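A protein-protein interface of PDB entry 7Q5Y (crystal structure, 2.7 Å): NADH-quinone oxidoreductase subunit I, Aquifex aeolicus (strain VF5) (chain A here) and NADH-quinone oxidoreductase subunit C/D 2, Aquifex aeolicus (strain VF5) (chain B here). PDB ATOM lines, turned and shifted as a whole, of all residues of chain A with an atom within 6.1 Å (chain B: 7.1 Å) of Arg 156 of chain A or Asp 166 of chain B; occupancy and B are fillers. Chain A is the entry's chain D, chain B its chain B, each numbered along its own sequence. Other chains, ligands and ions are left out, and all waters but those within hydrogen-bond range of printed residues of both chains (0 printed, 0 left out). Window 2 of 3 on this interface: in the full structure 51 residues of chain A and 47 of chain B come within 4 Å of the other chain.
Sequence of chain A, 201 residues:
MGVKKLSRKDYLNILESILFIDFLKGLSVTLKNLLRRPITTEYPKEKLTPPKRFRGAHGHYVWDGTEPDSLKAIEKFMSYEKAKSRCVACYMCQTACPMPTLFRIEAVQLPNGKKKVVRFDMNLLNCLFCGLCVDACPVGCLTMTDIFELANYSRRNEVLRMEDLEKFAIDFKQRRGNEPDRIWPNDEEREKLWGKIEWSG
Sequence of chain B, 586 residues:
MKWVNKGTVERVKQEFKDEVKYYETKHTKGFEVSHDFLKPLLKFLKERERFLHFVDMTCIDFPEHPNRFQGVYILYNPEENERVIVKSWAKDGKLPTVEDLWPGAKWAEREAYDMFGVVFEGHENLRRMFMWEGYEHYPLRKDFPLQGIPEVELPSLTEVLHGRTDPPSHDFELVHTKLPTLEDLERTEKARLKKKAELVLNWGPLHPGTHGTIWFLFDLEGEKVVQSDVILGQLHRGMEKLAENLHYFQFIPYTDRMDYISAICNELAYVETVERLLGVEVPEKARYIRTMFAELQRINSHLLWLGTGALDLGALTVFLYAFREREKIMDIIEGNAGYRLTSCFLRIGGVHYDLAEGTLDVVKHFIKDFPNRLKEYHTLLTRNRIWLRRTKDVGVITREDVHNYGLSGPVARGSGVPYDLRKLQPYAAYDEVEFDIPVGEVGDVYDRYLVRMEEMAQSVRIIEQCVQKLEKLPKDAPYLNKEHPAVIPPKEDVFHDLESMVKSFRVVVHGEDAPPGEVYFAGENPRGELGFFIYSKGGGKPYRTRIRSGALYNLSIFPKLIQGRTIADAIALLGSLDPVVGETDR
Printed residues of chain B within 4 Å of Val 159 of chain A: Ser 169 (3.8 Å).
Of the printed residues of chain A, Glu 159 of chain B touches Ser 154 and Arg 156.
Of the printed residues of chain A, Arg 164 of chain B touches Ser 154 and Arg 156.
Of chain A, only Arg 156 comes within 4 Å of Asp 166 of chain B.
Of the printed residues of chain A, Ser 169 of chain B touches Val 159.
The nearest residue of chain B that does not touch Arg 156 of chain A is Thr 165 of chain B (4.9 Å).
The nearest printed residue of chain A that does not touch Asp 166 of chain B is Arg 155 of chain A (8.5 Å).
Among the printed residues, merely in contact across the chains: Arg 155 of chain A with Pro 168 of chain B (3.8 Å), Arg 155 of chain A with Phe 172 of chain B (3.3 Å), Arg 156 of chain A with Pro 167 of chain B (3.7 Å), Arg 156 of chain A with Pro 168 of chain B (3.7 Å) and Val 159 of chain A with Ser 169 of chain B (3.8 Å).
OG of Ser 154 of chain A sits at hydrogen-bond distance from OE2 of Glu 159 of chain B, 3.0 Å away.
The guanidinium group (NE) of Arg 156 of chain A is in salt-bridge range of the side-chain carboxylate (OE1) of Glu 159 of chain B.
The side-chain hydroxyl (OG) of Ser 154 of chain A lies within hydrogen-bond range of the guanidinium group (NH1) of Arg 164 of chain B, at 3.0 Å.
The guanidinium group of Arg 156 of chain A is in salt-bridge range of the side-chain carboxylate of Asp 166 of chain B, at 3.3 Å.
The guanidinium group (NE) of Arg 156 of chain A lies close to the guanidinium group (NH1) of Arg 164 of chain B (3.3 Å).
Of the 7 printed residues of chain A, 4 touch a printed residue of chain B.
Of the 9 printed residues of chain B, 7 touch a printed residue of chain A.
Among the printed residues, 10 pairs touch across the chains.
OE1 of Glu 159 of chain B lies within salt-bridge range of NH1 of Arg 164 of chain B (2.8 Å).
The side-chain hydroxyl (OG) of Ser 154 of chain A sits close to the backbone NH (N) of Arg 156 of chain A (3.2 Å).
OD1 of Asn 157 of chain A sits at hydrogen-bond distance from N of Ser 154 of chain A (3.3 Å).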
ATOM      1  N   SER A 154      22.011  16.826  -6.115  1.00  0.00           N
ATOM      2  CA  SER A 154      22.179  18.141  -6.718  1.00  0.00           C
ATOM      3  C   SER A 154      23.643  18.538  -6.825  1.00  0.00           C
ATOM      4  O   SER A 154      24.462  18.213  -5.959  1.00  0.00           O
ATOM      5  CB  SER A 154      21.439  19.222  -5.931  1.00  0.00           C
ATOM      6  OG  SER A 154      21.805  20.503  -6.406  1.00  0.00           O
ATOM      7  N   ARG A 155      23.943  19.309  -7.876  1.00  0.00           N
ATOM      8  CA  ARG A 155      25.303  19.779  -8.062  1.00  0.00           C
ATOM      9  C   ARG A 155      25.817  20.443  -6.799  1.00  0.00           C
ATOM     10  O   ARG A 155      27.031  20.478  -6.556  1.00  0.00           O
ATOM     11  CB  ARG A 155      25.373  20.772  -9.223  1.00  0.00           C
ATOM     12  CG  ARG A 155      25.140  20.206 -10.599  1.00  0.00           C
ATOM     13  CD  ARG A 155      24.954  21.352 -11.548  1.00  0.00           C
ATOM     14  NE  ARG A 155      24.900  21.011 -12.965  1.00  0.00           N
ATOM     15  CZ  ARG A 155      25.843  21.347 -13.844  1.00  0.00           C
ATOM     16  NH1 ARG A 155      26.945  22.029 -13.467  1.00  0.00           N
ATOM     17  NH2 ARG A 155      25.682  21.012 -15.116  1.00  0.00           N
ATOM     18  N   ARG A 156      24.900  20.992  -5.994  1.00  0.00           N
ATOM     19  CA  ARG A 156      25.263  21.665  -4.750  1.00  0.00           C
ATOM     20  C   ARG A 156      25.799  20.698  -3.696  1.00  0.00           C
ATOM     21  O   ARG A 156      26.688  21.065  -2.917  1.00  0.00           O
ATOM     22  CB  ARG A 156      24.046  22.430  -4.211  1.00  0.00           C
ATOM     23  CG  ARG A 156      23.458  23.433  -5.211  1.00  0.00           C
ATOM     24  CD  ARG A 156      22.084  23.960  -4.805  1.00  0.00           C
ATOM     25  NE  ARG A 156      21.465  24.702  -5.907  1.00  0.00           N
ATOM     26  CZ  ARG A 156      21.618  26.012  -6.120  1.00  0.00           C
ATOM     27  NH1 ARG A 156      22.358  26.743  -5.290  1.00  0.00           N
ATOM     28  NH2 ARG A 156      21.028  26.596  -7.164  1.00  0.00           N
ATOM     29  N   ASN A 157      25.302  19.462  -3.657  1.00  0.00           N
ATOM     30  CA  ASN A 157      25.805  18.544  -2.646  1.00  0.00           C
ATOM     31  C   ASN A 157      27.196  18.042  -2.958  1.00  0.00           C
ATOM     32  O   ASN A 157      27.796  17.378  -2.108  1.00  0.00           O
ATOM     33  CB  ASN A 157      24.864  17.360  -2.467  1.00  0.00           C
ATOM     34  CG  ASN A 157      23.432  17.783  -2.290  1.00  0.00           C
ATOM     35  OD1 ASN A 157      22.520  17.175  -2.837  1.00  0.00           O
ATOM     36  ND2 ASN A 157      23.225  18.828  -1.514  1.00  0.00           N
ATOM     37  N   GLU A 158      27.709  18.336  -4.148  1.00  0.00           N
ATOM     38  CA  GLU A 158      29.033  17.912  -4.562  1.00  0.00           C
ATOM     39  C   GLU A 158      30.072  19.017  -4.418  1.00  0.00           C
ATOM     40  O   GLU A 158      31.157  18.916  -4.995  1.00  0.00           O
ATOM     41  CB  GLU A 158      28.976  17.403  -5.997  1.00  0.00           C
ATOM     42  CG  GLU A 158      27.894  16.360  -6.183  1.00  0.00           C
ATOM     43  CD  GLU A 158      28.054  15.229  -5.196  1.00  0.00           C
ATOM     44  OE1 GLU A 158      27.090  14.885  -4.493  1.00  0.00           O
ATOM     45  OE2 GLU A 158      29.168  14.700  -5.092  1.00  0.00           O
ATOM     46  N   VAL A 159      29.763  20.064  -3.656  1.00  0.00           N
ATOM     47  CA  VAL A 159      30.668  21.184  -3.425  1.00  0.00           C
ATOM     48  C   VAL A 159      31.103  21.102  -1.971  1.00  0.00           C
ATOM     49  O   VAL A 159      30.275  21.213  -1.056  1.00  0.00           O
ATOM     50  CB  VAL A 159      30.014  22.543  -3.737  1.00  0.00           C
ATOM     51  CG1 VAL A 159      30.930  23.711  -3.344  1.00  0.00           C
ATOM     52  CG2 VAL A 159      29.674  22.651  -5.204  1.00  0.00           C
ATOM     53  N   LEU A 160      32.395  20.874  -1.757  1.00  0.00           N
ATOM     54  CA  LEU A 160      32.930  20.758  -0.413  1.00  0.00           C
ATOM     55  C   LEU A 160      33.377  22.119   0.082  1.00  0.00           C
ATOM     56  O   LEU A 160      34.089  22.832  -0.624  1.00  0.00           O
ATOM     57  CB  LEU A 160      34.113  19.796  -0.381  1.00  0.00           C
ATOM     58  CG  LEU A 160      33.812  18.339  -0.753  1.00  0.00           C
ATOM     59  CD1 LEU A 160      35.125  17.541  -0.879  1.00  0.00           C
ATOM     60  CD2 LEU A 160      32.808  17.681   0.210  1.00  0.00           C
ATOM     61  N   GLU B 159      18.113  22.201 -11.437  1.00  0.00           N
ATOM     62  CA  GLU B 159      17.996  23.329 -10.518  1.00  0.00           C
ATOM     63  C   GLU B 159      16.744  24.153 -10.803  1.00  0.00           C
ATOM     64  O   GLU B 159      16.145  24.704  -9.873  1.00  0.00           O
ATOM     65  CB  GLU B 159      19.241  24.202 -10.603  1.00  0.00           C
ATOM     66  CG  GLU B 159      20.504  23.419 -10.339  1.00  0.00           C
ATOM     67  CD  GLU B 159      20.488  22.663  -9.027  1.00  0.00           C
ATOM     68  OE1 GLU B 159      20.264  23.319  -7.982  1.00  0.00           O
ATOM     69  OE2 GLU B 159      20.681  21.416  -9.055  1.00  0.00           O
ATOM     70  N   GLY B 163      13.062  25.436  -8.369  1.00  0.00           N
ATOM     71  CA  GLY B 163      12.997  26.851  -8.104  1.00  0.00           C
ATOM     72  C   GLY B 163      14.322  27.523  -7.844  1.00  0.00           C
ATOM     73  O   GLY B 163      14.394  28.749  -7.938  1.00  0.00           O
ATOM     74  N   ARG B 164      15.373  26.763  -7.524  1.00  0.00           N
ATOM     75  CA  ARG B 164      16.678  27.351  -7.274  1.00  0.00           C
ATOM     76  C   ARG B 164      17.182  27.988  -8.564  1.00  0.00           C
ATOM     77  O   ARG B 164      17.520  27.285  -9.522  1.00  0.00           O
ATOM     78  CB  ARG B 164      17.656  26.305  -6.747  1.00  0.00           C
ATOM     79  CG  ARG B 164      17.356  25.826  -5.339  1.00  0.00           C
ATOM     80  CD  ARG B 164      18.158  24.580  -5.027  1.00  0.00           C
ATOM     81  NE  ARG B 164      17.499  23.371  -5.520  1.00  0.00           N
ATOM     82  CZ  ARG B 164      18.128  22.221  -5.750  1.00  0.00           C
ATOM     83  NH1 ARG B 164      19.431  22.130  -5.548  1.00  0.00           N
ATOM     84  NH2 ARG B 164      17.463  21.168  -6.199  1.00  0.00           N
ATOM     85  N   THR B 165      17.213  29.320  -8.596  1.00  0.00           N
ATOM     86  CA  THR B 165      17.641  30.071  -9.767  1.00  0.00           C
ATOM     87  C   THR B 165      19.092  30.536  -9.703  1.00  0.00           C
ATOM     88  O   THR B 165      19.675  30.851 -10.749  1.00  0.00           O
ATOM     89  CB  THR B 165      16.718  31.275  -9.976  1.00  0.00           C
ATOM     90  OG1 THR B 165      16.583  31.999  -8.743  1.00  0.00           O
ATOM     91  CG2 THR B 165      15.354  30.805 -10.441  1.00  0.00           C
ATOM     92  N   ASP B 166      19.676  30.601  -8.510  1.00  0.00           N
ATOM     93  CA  ASP B 166      21.059  31.017  -8.354  1.00  0.00           C
ATOM     94  C   ASP B 166      22.007  29.927  -8.862  1.00  0.00           C
ATOM     95  O   ASP B 166      21.660  28.740  -8.871  1.00  0.00           O
ATOM     96  CB  ASP B 166      21.333  31.321  -6.883  1.00  0.00           C
ATOM     97  CG  ASP B 166      20.777  30.255  -5.953  1.00  0.00           C
ATOM     98  OD1 ASP B 166      19.783  29.578  -6.315  1.00  0.00           O
ATOM     99  OD2 ASP B 166      21.337  30.094  -4.850  1.00  0.00           O
ATOM    100  N   PRO B 167      23.219  30.301  -9.273  1.00  0.00           N
ATOM    101  CA  PRO B 167      24.177  29.301  -9.787  1.00  0.00           C
ATOM    102  C   PRO B 167      24.459  28.239  -8.740  1.00  0.00           C
ATOM    103  O   PRO B 167      24.640  28.552  -7.553  1.00  0.00           O
ATOM    104  CB  PRO B 167      25.425  30.137 -10.107  1.00  0.00           C
ATOM    105  CG  PRO B 167      25.266  31.381  -9.303  1.00  0.00           C
ATOM    106  CD  PRO B 167      23.795  31.656  -9.268  1.00  0.00           C
ATOM    107  N   PRO B 168      24.505  26.963  -9.141  1.00  0.00           N
ATOM    108  CA  PRO B 168      24.712  25.888  -8.152  1.00  0.00           C
ATOM    109  C   PRO B 168      26.142  25.720  -7.689  1.00  0.00           C
ATOM    110  O   PRO B 168      26.370  25.179  -6.595  1.00  0.00           O
ATOM    111  CB  PRO B 168      24.218  24.643  -8.897  1.00  0.00           C
ATOM    112  CG  PRO B 168      24.490  24.957 -10.374  1.00  0.00           C
ATOM    113  CD  PRO B 168      24.416  26.458 -10.530  1.00  0.00           C
ATOM    114  N   SER B 169      27.104  26.193  -8.464  1.00  0.00           N
ATOM    115  CA  SER B 169      28.497  26.084  -8.104  1.00  0.00           C
ATOM    116  C   SER B 169      29.208  27.361  -8.493  1.00  0.00           C
ATOM    117  O   SER B 169      28.837  28.011  -9.471  1.00  0.00           O
ATOM    118  CB  SER B 169      29.158  24.909  -8.800  1.00  0.00           C
ATOM    119  OG  SER B 169      30.462  24.755  -8.294  1.00  0.00           O
ATOM    120  N   PHE B 172      29.984  27.449 -12.109  1.00  0.00           N
ATOM    121  CA  PHE B 172      28.944  27.108 -13.072  1.00  0.00           C
ATOM    122  C   PHE B 172      28.749  28.277 -14.021  1.00  0.00           C
ATOM    123  O   PHE B 172      28.383  29.376 -13.590  1.00  0.00           O
ATOM    124  CB  PHE B 172      27.615  26.768 -12.409  1.00  0.00           C
ATOM    125  CG  PHE B 172      26.509  26.491 -13.405  1.00  0.00           C
ATOM    126  CD1 PHE B 172      26.305  25.213 -13.897  1.00  0.00           C
ATOM    127  CD2 PHE B 172      25.685  27.506 -13.856  1.00  0.00           C
ATOM    128  CE1 PHE B 172      25.297  24.953 -14.820  1.00  0.00           C
ATOM    129  CE2 PHE B 172      24.705  27.267 -14.767  1.00  0.00           C
ATOM    130  CZ  PHE B 172      24.496  25.975 -15.250  1.00  0.00           C
